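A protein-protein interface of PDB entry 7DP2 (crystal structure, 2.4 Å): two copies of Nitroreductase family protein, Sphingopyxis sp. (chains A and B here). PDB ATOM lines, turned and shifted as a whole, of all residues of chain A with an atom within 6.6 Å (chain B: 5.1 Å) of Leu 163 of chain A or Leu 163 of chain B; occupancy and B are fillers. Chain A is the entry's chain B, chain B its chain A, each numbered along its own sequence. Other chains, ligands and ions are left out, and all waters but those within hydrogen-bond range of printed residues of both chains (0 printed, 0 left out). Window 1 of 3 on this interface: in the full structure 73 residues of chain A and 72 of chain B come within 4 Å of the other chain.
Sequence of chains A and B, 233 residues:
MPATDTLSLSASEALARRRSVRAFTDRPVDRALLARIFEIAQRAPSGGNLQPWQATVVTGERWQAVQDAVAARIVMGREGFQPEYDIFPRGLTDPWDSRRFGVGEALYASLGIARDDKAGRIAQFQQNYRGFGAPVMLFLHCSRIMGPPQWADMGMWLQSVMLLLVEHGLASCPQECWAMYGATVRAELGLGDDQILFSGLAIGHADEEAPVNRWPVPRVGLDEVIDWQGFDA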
ATOM      1  N   LEU A   9      -3.721   4.777   5.216  1.00  0.00           N
ATOM      2  CA  LEU A   9      -4.750   3.751   5.397  1.00  0.00           C
ATOM      3  C   LEU A   9      -4.122   2.356   5.596  1.00  0.00           C
ATOM      4  O   LEU A   9      -3.353   1.882   4.746  1.00  0.00           O
ATOM      5  CB  LEU A   9      -5.710   3.754   4.194  1.00  0.00           C
ATOM      6  CG  LEU A   9      -7.073   3.049   4.245  1.00  0.00           C
ATOM      7  CD1 LEU A   9      -8.083   3.851   5.063  1.00  0.00           C
ATOM      8  CD2 LEU A   9      -7.612   2.853   2.849  1.00  0.00           C
ATOM      9  N   ALA A  11      -3.673  -1.853   6.152  1.00  0.00           N
ATOM     10  CA  ALA A  11      -4.071  -3.031   5.386  1.00  0.00           C
ATOM     11  C   ALA A  11      -5.454  -3.552   5.803  1.00  0.00           C
ATOM     12  O   ALA A  11      -6.270  -3.895   4.954  1.00  0.00           O
ATOM     13  CB  ALA A  11      -3.022  -4.122   5.522  1.00  0.00           C
ATOM     14  N   ALA A  14      -7.831  -1.107   4.321  1.00  0.00           N
ATOM     15  CA  ALA A  14      -7.842  -1.339   2.878  1.00  0.00           C
ATOM     16  C   ALA A  14      -8.703  -2.554   2.496  1.00  0.00           C
ATOM     17  O   ALA A  14      -9.529  -2.470   1.593  1.00  0.00           O
ATOM     18  CB  ALA A  14      -6.426  -1.520   2.369  1.00  0.00           C
ATOM     19  N   LEU A  15      -8.539  -3.659   3.221  1.00  0.00           N
ATOM     20  CA  LEU A  15      -9.327  -4.878   2.981  1.00  0.00           C
ATOM     21  C   LEU A  15     -10.783  -4.656   3.264  1.00  0.00           C
ATOM     22  O   LEU A  15     -11.629  -5.074   2.505  1.00  0.00           O
ATOM     23  CB  LEU A  15      -8.826  -6.035   3.854  1.00  0.00           C
ATOM     24  CG  LEU A  15      -7.775  -6.983   3.270  1.00  0.00           C
ATOM     25  CD1 LEU A  15      -7.213  -7.840   4.376  1.00  0.00           C
ATOM     26  CD2 LEU A  15      -8.348  -7.879   2.191  1.00  0.00           C
ATOM     27  N   ALA A  16     -11.060  -3.955   4.355  1.00  0.00           N
ATOM     28  CA  ALA A  16     -12.405  -3.643   4.759  1.00  0.00           C
ATOM     29  C   ALA A  16     -13.127  -2.749   3.752  1.00  0.00           C
ATOM     30  O   ALA A  16     -14.354  -2.776   3.647  1.00  0.00           O
ATOM     31  CB  ALA A  16     -12.393  -2.960   6.131  1.00  0.00           C
ATOM     32  N   ARG A  18     -12.198  -2.302   0.394  1.00  0.00           N
ATOM     33  CA  ARG A  18     -12.246  -2.779  -0.973  1.00  0.00           C
ATOM     34  C   ARG A  18     -13.565  -3.492  -1.191  1.00  0.00           C
ATOM     35  O   ARG A  18     -13.900  -4.409  -0.450  1.00  0.00           O
ATOM     36  CB  ARG A  18     -11.093  -3.738  -1.289  1.00  0.00           C
ATOM     37  CG  ARG A  18     -11.055  -4.186  -2.727  1.00  0.00           C
ATOM     38  CD  ARG A  18     -10.808  -5.746  -2.846  1.00  0.00           C
ATOM     39  NE  ARG A  18     -11.839  -6.528  -2.162  1.00  0.00           N
ATOM     40  CZ  ARG A  18     -13.036  -6.836  -2.669  1.00  0.00           C
ATOM     41  NH1 ARG A  18     -13.351  -6.470  -3.901  1.00  0.00           N
ATOM     42  NH2 ARG A  18     -13.923  -7.517  -1.939  1.00  0.00           N
ATOM     43  N   LEU A 158      -3.345  -9.904  -8.009  1.00  0.00           N
ATOM     44  CA  LEU A 158      -4.560  -9.153  -8.266  1.00  0.00           C
ATOM     45  C   LEU A 158      -5.135  -8.520  -6.994  1.00  0.00           C
ATOM     46  O   LEU A 158      -5.537  -7.340  -6.988  1.00  0.00           O
ATOM     47  CB  LEU A 158      -5.605 -10.054  -8.932  1.00  0.00           C
ATOM     48  CG  LEU A 158      -6.784  -9.287  -9.539  1.00  0.00           C
ATOM     49  CD1 LEU A 158      -6.251  -8.297 -10.592  1.00  0.00           C
ATOM     50  CD2 LEU A 158      -7.883 -10.210 -10.129  1.00  0.00           C
ATOM     51  N   GLN A 159      -5.190  -9.309  -5.925  1.00  0.00           N
ATOM     52  CA  GLN A 159      -5.667  -8.802  -4.655  1.00  0.00           C
ATOM     53  C   GLN A 159      -4.732  -7.697  -4.153  1.00  0.00           C
ATOM     54  O   GLN A 159      -5.186  -6.700  -3.602  1.00  0.00           O
ATOM     55  CB  GLN A 159      -5.776  -9.913  -3.617  1.00  0.00           C
ATOM     56  CG  GLN A 159      -6.088  -9.361  -2.225  1.00  0.00           C
ATOM     57  CD  GLN A 159      -7.515  -8.833  -2.048  1.00  0.00           C
ATOM     58  OE1 GLN A 159      -8.185  -8.392  -2.996  1.00  0.00           O
ATOM     59  NE2 GLN A 159      -7.984  -8.885  -0.818  1.00  0.00           N
ATOM     60  N   SER A 160      -3.430  -7.877  -4.373  1.00  0.00           N
ATOM     61  CA  SER A 160      -2.468  -6.824  -4.070  1.00  0.00           C
ATOM     62  C   SER A 160      -2.820  -5.527  -4.784  1.00  0.00           C
ATOM     63  O   SER A 160      -2.855  -4.471  -4.165  1.00  0.00           O
ATOM     64  CB  SER A 160      -1.040  -7.226  -4.459  1.00  0.00           C
ATOM     65  OG  SER A 160      -0.566  -8.346  -3.738  1.00  0.00           O
ATOM     66  N   VAL A 161      -3.078  -5.618  -6.081  1.00  0.00           N
ATOM     67  CA  VAL A 161      -3.430  -4.450  -6.880  1.00  0.00           C
ATOM     68  C   VAL A 161      -4.688  -3.769  -6.335  1.00  0.00           C
ATOM     69  O   VAL A 161      -4.719  -2.546  -6.177  1.00  0.00           O
ATOM     70  CB  VAL A 161      -3.636  -4.845  -8.352  1.00  0.00           C
ATOM     71  CG1 VAL A 161      -4.163  -3.682  -9.194  1.00  0.00           C
ATOM     72  CG2 VAL A 161      -2.343  -5.377  -8.928  1.00  0.00           C
ATOM     73  N   MET A 162      -5.703  -4.570  -6.011  1.00  0.00           N
ATOM     74  CA  MET A 162      -6.982  -4.029  -5.548  1.00  0.00           C
ATOM     75  C   MET A 162      -6.874  -3.319  -4.191  1.00  0.00           C
ATOM     76  O   MET A 162      -7.483  -2.268  -3.981  1.00  0.00           O
ATOM     77  CB  MET A 162      -8.054  -5.140  -5.488  1.00  0.00           C
ATOM     78  CG  MET A 162      -8.419  -5.679  -6.889  1.00  0.00           C
ATOM     79  SD  MET A 162      -9.708  -6.936  -6.929  1.00  0.00           S
ATOM     80  CE  MET A 162      -8.866  -8.486  -6.689  1.00  0.00           C
ATOM     81  N   LEU A 163      -6.068  -3.864  -3.290  1.00  0.00           N
ATOM     82  CA  LEU A 163      -5.817  -3.208  -2.005  1.00  0.00           C
ATOM     83  C   LEU A 163      -5.078  -1.896  -2.164  1.00  0.00           C
ATOM     84  O   LEU A 163      -5.329  -0.960  -1.412  1.00  0.00           O
ATOM     85  CB  LEU A 163      -5.027  -4.126  -1.084  1.00  0.00           C
ATOM     86  CG  LEU A 163      -5.824  -5.364  -0.703  1.00  0.00           C
ATOM     87  CD1 LEU A 163      -5.017  -6.222   0.240  1.00  0.00           C
ATOM     88  CD2 LEU A 163      -7.176  -4.942  -0.083  1.00  0.00           C
ATOM     89  N   LEU A 164      -4.152  -1.832  -3.122  1.00  0.00           N
ATOM     90  CA  LEU A 164      -3.394  -0.597  -3.371  1.00  0.00           C
ATOM     91  C   LEU A 164      -4.244   0.508  -3.976  1.00  0.00           C
ATOM     92  O   LEU A 164      -4.049   1.687  -3.679  1.00  0.00           O
ATOM     93  CB  LEU A 164      -2.189  -0.865  -4.267  1.00  0.00           C
ATOM     94  CG  LEU A 164      -1.024  -1.573  -3.554  1.00  0.00           C
ATOM     95  CD1 LEU A 164      -0.056  -2.282  -4.528  1.00  0.00           C
ATOM     96  CD2 LEU A 164      -0.264  -0.568  -2.688  1.00  0.00           C
ATOM     97  N   LEU A 165      -5.168   0.127  -4.851  1.00  0.00           N
ATOM     98  CA  LEU A 165      -6.103   1.077  -5.430  1.00  0.00           C
ATOM     99  C   LEU A 165      -6.865   1.796  -4.327  1.00  0.00           C
ATOM    100  O   LEU A 165      -6.932   3.026  -4.289  1.00  0.00           O
ATOM    101  CB  LEU A 165      -7.064   0.360  -6.359  1.00  0.00           C
ATOM    102  CG  LEU A 165      -6.258  -0.160  -7.540  1.00  0.00           C
ATOM    103  CD1 LEU A 165      -7.112  -1.004  -8.483  1.00  0.00           C
ATOM    104  CD2 LEU A 165      -5.584   0.998  -8.260  1.00  0.00           C
ATOM    105  N   VAL A 166      -7.427   1.009  -3.423  1.00  0.00           N
ATOM    106  CA  VAL A 166      -8.189   1.556  -2.323  1.00  0.00           C
ATOM    107  C   VAL A 166      -7.317   2.483  -1.467  1.00  0.00           C
ATOM    108  O   VAL A 166      -7.672   3.628  -1.219  1.00  0.00           O
ATOM    109  CB  VAL A 166      -8.769   0.416  -1.473  1.00  0.00           C
ATOM    110  CG1 VAL A 166      -9.498   0.962  -0.254  1.00  0.00           C
ATOM    111  CG2 VAL A 166      -9.694  -0.431  -2.331  1.00  0.00           C
ATOM    112  N   GLU A 167      -6.158   1.997  -1.043  1.00  0.00           N
ATOM    113  CA  GLU A 167      -5.267   2.817  -0.229  1.00  0.00           C
ATOM    114  C   GLU A 167      -4.972   4.171  -0.885  1.00  0.00           C
ATOM    115  O   GLU A 167      -4.779   5.178  -0.197  1.00  0.00           O
ATOM    116  CB  GLU A 167      -3.959   2.086   0.078  1.00  0.00           C
ATOM    117  CG  GLU A 167      -2.951   2.995   0.785  1.00  0.00           C
ATOM    118  CD  GLU A 167      -1.724   2.264   1.244  1.00  0.00           C
ATOM    119  OE1 GLU A 167      -0.661   2.444   0.627  1.00  0.00           O
ATOM    120  OE2 GLU A 167      -1.828   1.507   2.227  1.00  0.00           O
ATOM    121  N   HIS A 168      -4.943   4.185  -2.213  1.00  0.00           N
ATOM    122  CA  HIS A 168      -4.622   5.402  -2.947  1.00  0.00           C
ATOM    123  C   HIS A 168      -5.854   6.111  -3.529  1.00  0.00           C
ATOM    124  O   HIS A 168      -5.745   6.884  -4.470  1.00  0.00           O
ATOM    125  CB  HIS A 168      -3.626   5.077  -4.059  1.00  0.00           C
ATOM    126  CG  HIS A 168      -2.269   4.709  -3.523  1.00  0.00           C
ATOM    127  ND1 HIS A 168      -1.125   4.793  -4.304  1.00  0.00           N
ATOM    128  CD2 HIS A 168      -1.874   4.297  -2.318  1.00  0.00           C
ATOM    129  CE1 HIS A 168      -0.086   4.431  -3.574  1.00  0.00           C
ATOM    130  NE2 HIS A 168      -0.506   4.120  -2.358  1.00  0.00           N
ATOM    131  N   SER A 172     -11.864  -0.399  -7.917  1.00  0.00           N
ATOM    132  CA  SER A 172     -11.806  -1.408  -8.969  1.00  0.00           C
ATOM    133  C   SER A 172     -12.970  -2.382  -8.967  1.00  0.00           C
ATOM    134  O   SER A 172     -13.743  -2.446  -8.011  1.00  0.00           O
ATOM    135  CB  SER A 172     -10.516  -2.223  -8.855  1.00  0.00           C
ATOM    136  OG  SER A 172     -10.538  -3.012  -7.681  1.00  0.00           O
ATOM    137  N   ALA B  11      -1.168  -0.630   3.915  1.00  0.00           N
ATOM    138  CA  ALA B  11      -1.214  -1.754   2.987  1.00  0.00           C
ATOM    139  C   ALA B  11       0.081  -1.833   2.184  1.00  0.00           C
ATOM    140  O   ALA B  11       0.647  -2.908   2.004  1.00  0.00           O
ATOM    141  CB  ALA B  11      -2.400  -1.632   2.060  1.00  0.00           C
ATOM    142  N   ALA B  14       2.871  -3.089   4.622  1.00  0.00           N
ATOM    143  CA  ALA B  14       2.697  -4.511   4.885  1.00  0.00           C
ATOM    144  C   ALA B  14       3.104  -5.303   3.653  1.00  0.00           C
ATOM    145  O   ALA B  14       3.789  -6.298   3.752  1.00  0.00           O
ATOM    146  CB  ALA B  14       1.266  -4.823   5.279  1.00  0.00           C
ATOM    147  N   LEU B  15       2.688  -4.833   2.489  1.00  0.00           N
ATOM    148  CA  LEU B  15       3.040  -5.491   1.245  1.00  0.00           C
ATOM    149  C   LEU B  15       4.544  -5.424   1.001  1.00  0.00           C
ATOM    150  O   LEU B  15       5.147  -6.377   0.543  1.00  0.00           O
ATOM    151  CB  LEU B  15       2.286  -4.856   0.092  1.00  0.00           C
ATOM    152  CG  LEU B  15       2.170  -5.677  -1.184  1.00  0.00           C
ATOM    153  CD1 LEU B  15       1.255  -6.875  -0.970  1.00  0.00           C
ATOM    154  CD2 LEU B  15       1.647  -4.795  -2.299  1.00  0.00           C
ATOM    155  N   ARG B  18       6.026  -7.901   3.661  1.00  0.00           N
ATOM    156  CA  ARG B  18       5.770  -9.333   3.594  1.00  0.00           C
ATOM    157  C   ARG B  18       6.853 -10.031   2.785  1.00  0.00           C
ATOM    158  O   ARG B  18       7.161  -9.619   1.674  1.00  0.00           O
ATOM    159  CB  ARG B  18       4.401  -9.638   2.983  1.00  0.00           C
ATOM    160  CG  ARG B  18       4.070 -11.112   3.032  1.00  0.00           C
ATOM    161  CD  ARG B  18       3.442 -11.610   1.739  1.00  0.00           C
ATOM    162  NE  ARG B  18       4.289 -11.332   0.588  1.00  0.00           N
ATOM    163  CZ  ARG B  18       5.351 -12.051   0.215  1.00  0.00           C
ATOM    164  NH1 ARG B  18       5.745 -13.114   0.922  1.00  0.00           N
ATOM    165  NH2 ARG B  18       6.034 -11.683  -0.867  1.00  0.00           N
ATOM    166  N   GLN B 159      -3.203 -14.205   0.058  1.00  0.00           N
ATOM    167  CA  GLN B 159      -2.416 -12.988   0.129  1.00  0.00           C
ATOM    168  C   GLN B 159      -2.957 -12.023   1.174  1.00  0.00           C
ATOM    169  O   GLN B 159      -2.192 -11.355   1.859  1.00  0.00           O
ATOM    170  CB  GLN B 159      -2.355 -12.301  -1.227  1.00  0.00           C
ATOM    171  CG  GLN B 159      -1.740 -10.901  -1.215  1.00  0.00           C
ATOM    172  CD  GLN B 159      -0.230 -10.895  -0.955  1.00  0.00           C
ATOM    173  OE1 GLN B 159       0.328 -11.765  -0.266  1.00  0.00           O
ATOM    174  NE2 GLN B 159       0.438  -9.922  -1.536  1.00  0.00           N
ATOM    175  N   SER B 160      -4.276 -11.954   1.303  1.00  0.00           N
ATOM    176  CA  SER B 160      -4.875 -11.139   2.353  1.00  0.00           C
ATOM    177  C   SER B 160      -4.344 -11.578   3.732  1.00  0.00           C
ATOM    178  O   SER B 160      -3.886 -10.766   4.545  1.00  0.00           O
ATOM    179  CB  SER B 160      -6.382 -11.253   2.296  1.00  0.00           C
ATOM    180  OG  SER B 160      -6.864 -10.846   1.022  1.00  0.00           O
ATOM    181  N   VAL B 161      -4.374 -12.880   3.969  1.00  0.00           N
ATOM    182  CA  VAL B 161      -3.941 -13.433   5.243  1.00  0.00           C
ATOM    183  C   VAL B 161      -2.493 -13.043   5.531  1.00  0.00           C
ATOM    184  O   VAL B 161      -2.162 -12.641   6.638  1.00  0.00           O
ATOM    185  CB  VAL B 161      -4.120 -14.964   5.239  1.00  0.00           C
ATOM    186  CG1 VAL B 161      -3.538 -15.614   6.491  1.00  0.00           C
ATOM    187  CG2 VAL B 161      -5.606 -15.306   5.083  1.00  0.00           C
ATOM    188  N   MET B 162      -1.636 -13.146   4.526  1.00  0.00           N
ATOM    189  CA  MET B 162      -0.221 -12.850   4.723  1.00  0.00           C
ATOM    190  C   MET B 162       0.014 -11.361   5.036  1.00  0.00           C
ATOM    191  O   MET B 162       0.813 -11.008   5.900  1.00  0.00           O
ATOM    192  CB  MET B 162       0.586 -13.293   3.487  1.00  0.00           C
ATOM    193  CG  MET B 162       0.632 -14.833   3.289  1.00  0.00           C
ATOM    194  SD  MET B 162       1.578 -15.392   1.851  1.00  0.00           S
ATOM    195  CE  MET B 162       0.373 -15.439   0.545  1.00  0.00           C
ATOM    196  N   LEU B 163      -0.726 -10.487   4.374  1.00  0.00           N
ATOM    197  CA  LEU B 163      -0.624  -9.073   4.667  1.00  0.00           C
ATOM    198  C   LEU B 163      -1.115  -8.699   6.068  1.00  0.00           C
ATOM    199  O   LEU B 163      -0.494  -7.890   6.734  1.00  0.00           O
ATOM    200  CB  LEU B 163      -1.402  -8.282   3.628  1.00  0.00           C
ATOM    201  CG  LEU B 163      -0.802  -8.447   2.238  1.00  0.00           C
ATOM    202  CD1 LEU B 163      -1.546  -7.551   1.257  1.00  0.00           C
ATOM    203  CD2 LEU B 163       0.708  -8.117   2.266  1.00  0.00           C
ATOM    204  N   LEU B 164      -2.197  -9.320   6.531  1.00  0.00           N
ATOM    205  CA  LEU B 164      -2.732  -9.008   7.854  1.00  0.00           C
ATOM    206  C   LEU B 164      -1.748  -9.466   8.920  1.00  0.00           C
ATOM    207  O   LEU B 164      -1.559  -8.790   9.921  1.00  0.00           O
ATOM    208  CB  LEU B 164      -4.092  -9.686   8.068  1.00  0.00           C
ATOM    209  CG  LEU B 164      -5.211  -9.078   7.219  1.00  0.00           C
ATOM    210  CD1 LEU B 164      -6.409 -10.034   6.994  1.00  0.00           C
ATOM    211  CD2 LEU B 164      -5.649  -7.756   7.793  1.00  0.00           C
ATOM    212  N   LEU B 165      -1.129 -10.619   8.678  1.00  0.00           N
ATOM    213  CA  LEU B 165      -0.124 -11.167   9.564  1.00  0.00           C
ATOM    214  C   LEU B 165       0.977 -10.183   9.804  1.00  0.00           C
ATOM    215  O   LEU B 165       1.325  -9.897  10.955  1.00  0.00           O
ATOM    216  CB  LEU B 165       0.482 -12.453   9.001  1.00  0.00           C
ATOM    217  CG  LEU B 165      -0.415 -13.693   8.955  1.00  0.00           C
ATOM    218  CD1 LEU B 165       0.320 -14.840   8.281  1.00  0.00           C
ATOM    219  CD2 LEU B 165      -0.900 -14.093  10.344  1.00  0.00           C
ATOM    220  N   VAL B 166       1.517  -9.661   8.713  1.00  0.00           N
ATOM    221  CA  VAL B 166       2.614  -8.712   8.799  1.00  0.00           C
ATOM    222  C   VAL B 166       2.152  -7.543   9.630  1.00  0.00           C
ATOM    223  O   VAL B 166       2.800  -7.169  10.614  1.00  0.00           O
ATOM    224  CB  VAL B 166       3.072  -8.216   7.416  1.00  0.00           C
ATOM    225  CG1 VAL B 166       4.145  -7.159   7.571  1.00  0.00           C
ATOM    226  CG2 VAL B 166       3.588  -9.367   6.577  1.00  0.00           C
ATOM    227  N   GLU B 167       0.987  -7.021   9.265  1.00  0.00           N
ATOM    228  CA  GLU B 167       0.406  -5.883   9.951  1.00  0.00           C
ATOM    229  C   GLU B 167       0.363  -6.092  11.454  1.00  0.00           C
ATOM    230  O   GLU B 167       0.560  -5.148  12.218  1.00  0.00           O
ATOM    231  CB  GLU B 167      -1.012  -5.615   9.430  1.00  0.00           C
ATOM    232  CG  GLU B 167      -1.739  -4.541  10.228  1.00  0.00           C
ATOM    233  CD  GLU B 167      -3.096  -4.201   9.652  1.00  0.00           C
ATOM    234  OE1 GLU B 167      -4.111  -4.545  10.295  1.00  0.00           O
ATOM    235  OE2 GLU B 167      -3.145  -3.566   8.574  1.00  0.00           O
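Of chain A, only Leu 163 comes within 4 Å of Leu 163 of chain B.
Printed residues of chain B within 4 Å of Leu 9 of chain A: Ala 11 (3.4 Å).
Of the printed residues of chain B, Glu 167 of chain A touches Ala 11.
Of the printed residues of chain B, Ala 11 of chain A touches Ala 11 (3.6 Å) and Glu 167 (3.0 Å).
Of the printed residues of chain A, Gln 159 of chain B touches Ser 160.
Leu 165 of chain A touches none of the printed residues of chain B.
The nearest printed residue of chain A that does not touch Leu 164 of chain B is Ala 11 of chain A (4.7 Å).
Among the printed residues, pairs that only touch across the chains: Leu 15 of chain A with Leu 164 of chain B, Leu 15 of chain A with Ser 160 of chain B, Ala 11 of chain A with Ala 11 of chain B, Ser 160 of chain A with Leu 15 of chain B, Leu 164 of chain A with Leu 15 of chain B and Leu 163 of chain A with Leu 163 of chain B.
Of the 18 printed residues of chain A, 8 touch a printed residue of chain B.
Printed residues of chain A that touch a printed residue of chain B: Leu 9, Ala 11, Leu 15, Gln 159, Ser 160, Leu 163, Leu 164 and Glu 167.
Hydrophobic or aromatic side chains of chain A within 4 Å of the printed part of chain B: Ala 11, Leu 15, Leu 163 and Leu 164.
Of the 13 printed residues of chain B, 7 touch a printed residue of chain A.
Hydrophobic or aromatic side chains of chain B that line the printed part of chain A: Ala 11, Leu 15, Leu 163 and Leu 164.
Among the printed residues, 11 pairs touch across the chains.
Ala 11 of chain B touches its own counterpart, Ala 11 of chain A.
Leu 15 of chain A touches Ser 160 of chain B, and with the chains exchanged Ser 160 of chain A touches Leu 15 of chain B.
Leu 15 of chain A touches Leu 164 of chain B, and with the chains exchanged Leu 164 of chain A touches Leu 15 of chain B.
Leu 163 of chain A touches its own counterpart, Leu 163 of chain B.
Positions printed for both chains: 11, 14, 15, 18, 159, 160, 161, 162, 163, 164, 165, 166 and 167.
Of the 11 pairs that touch across the chains among the printed residues, 10 have their exchanged pair printed and touching as well.
The side-chain carboxylate (OE1) of Glu 167 of chain A sits at hydrogen-bond distance from a ring nitrogen (NE2) of His 168 of chain A (3.4 Å).
N of Ala 11 of chain B is in hydrogen-bond range of O of Leu 9 of chain A, at 3.4 Å.
OE2 of Glu 167 of chain A lies within hydrogen-bond range of N of Ala 11 of chain B (2.8 Å).
The side-chain amide nitrogen of Gln 159 of chain B is in hydrogen-bond range of the side-chain hydroxyl of Ser 160 of chain A (2.9 Å).
NE2 of Gln 159 of chain A lies within hydrogen-bond range of OG of Ser 160 of chain B, 2.9 Å away.
The side-chain carboxylate (OE2) of Glu 167 of chain B sits at hydrogen-bond distance from the backbone NH (N) of Ala 11 of chain A.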
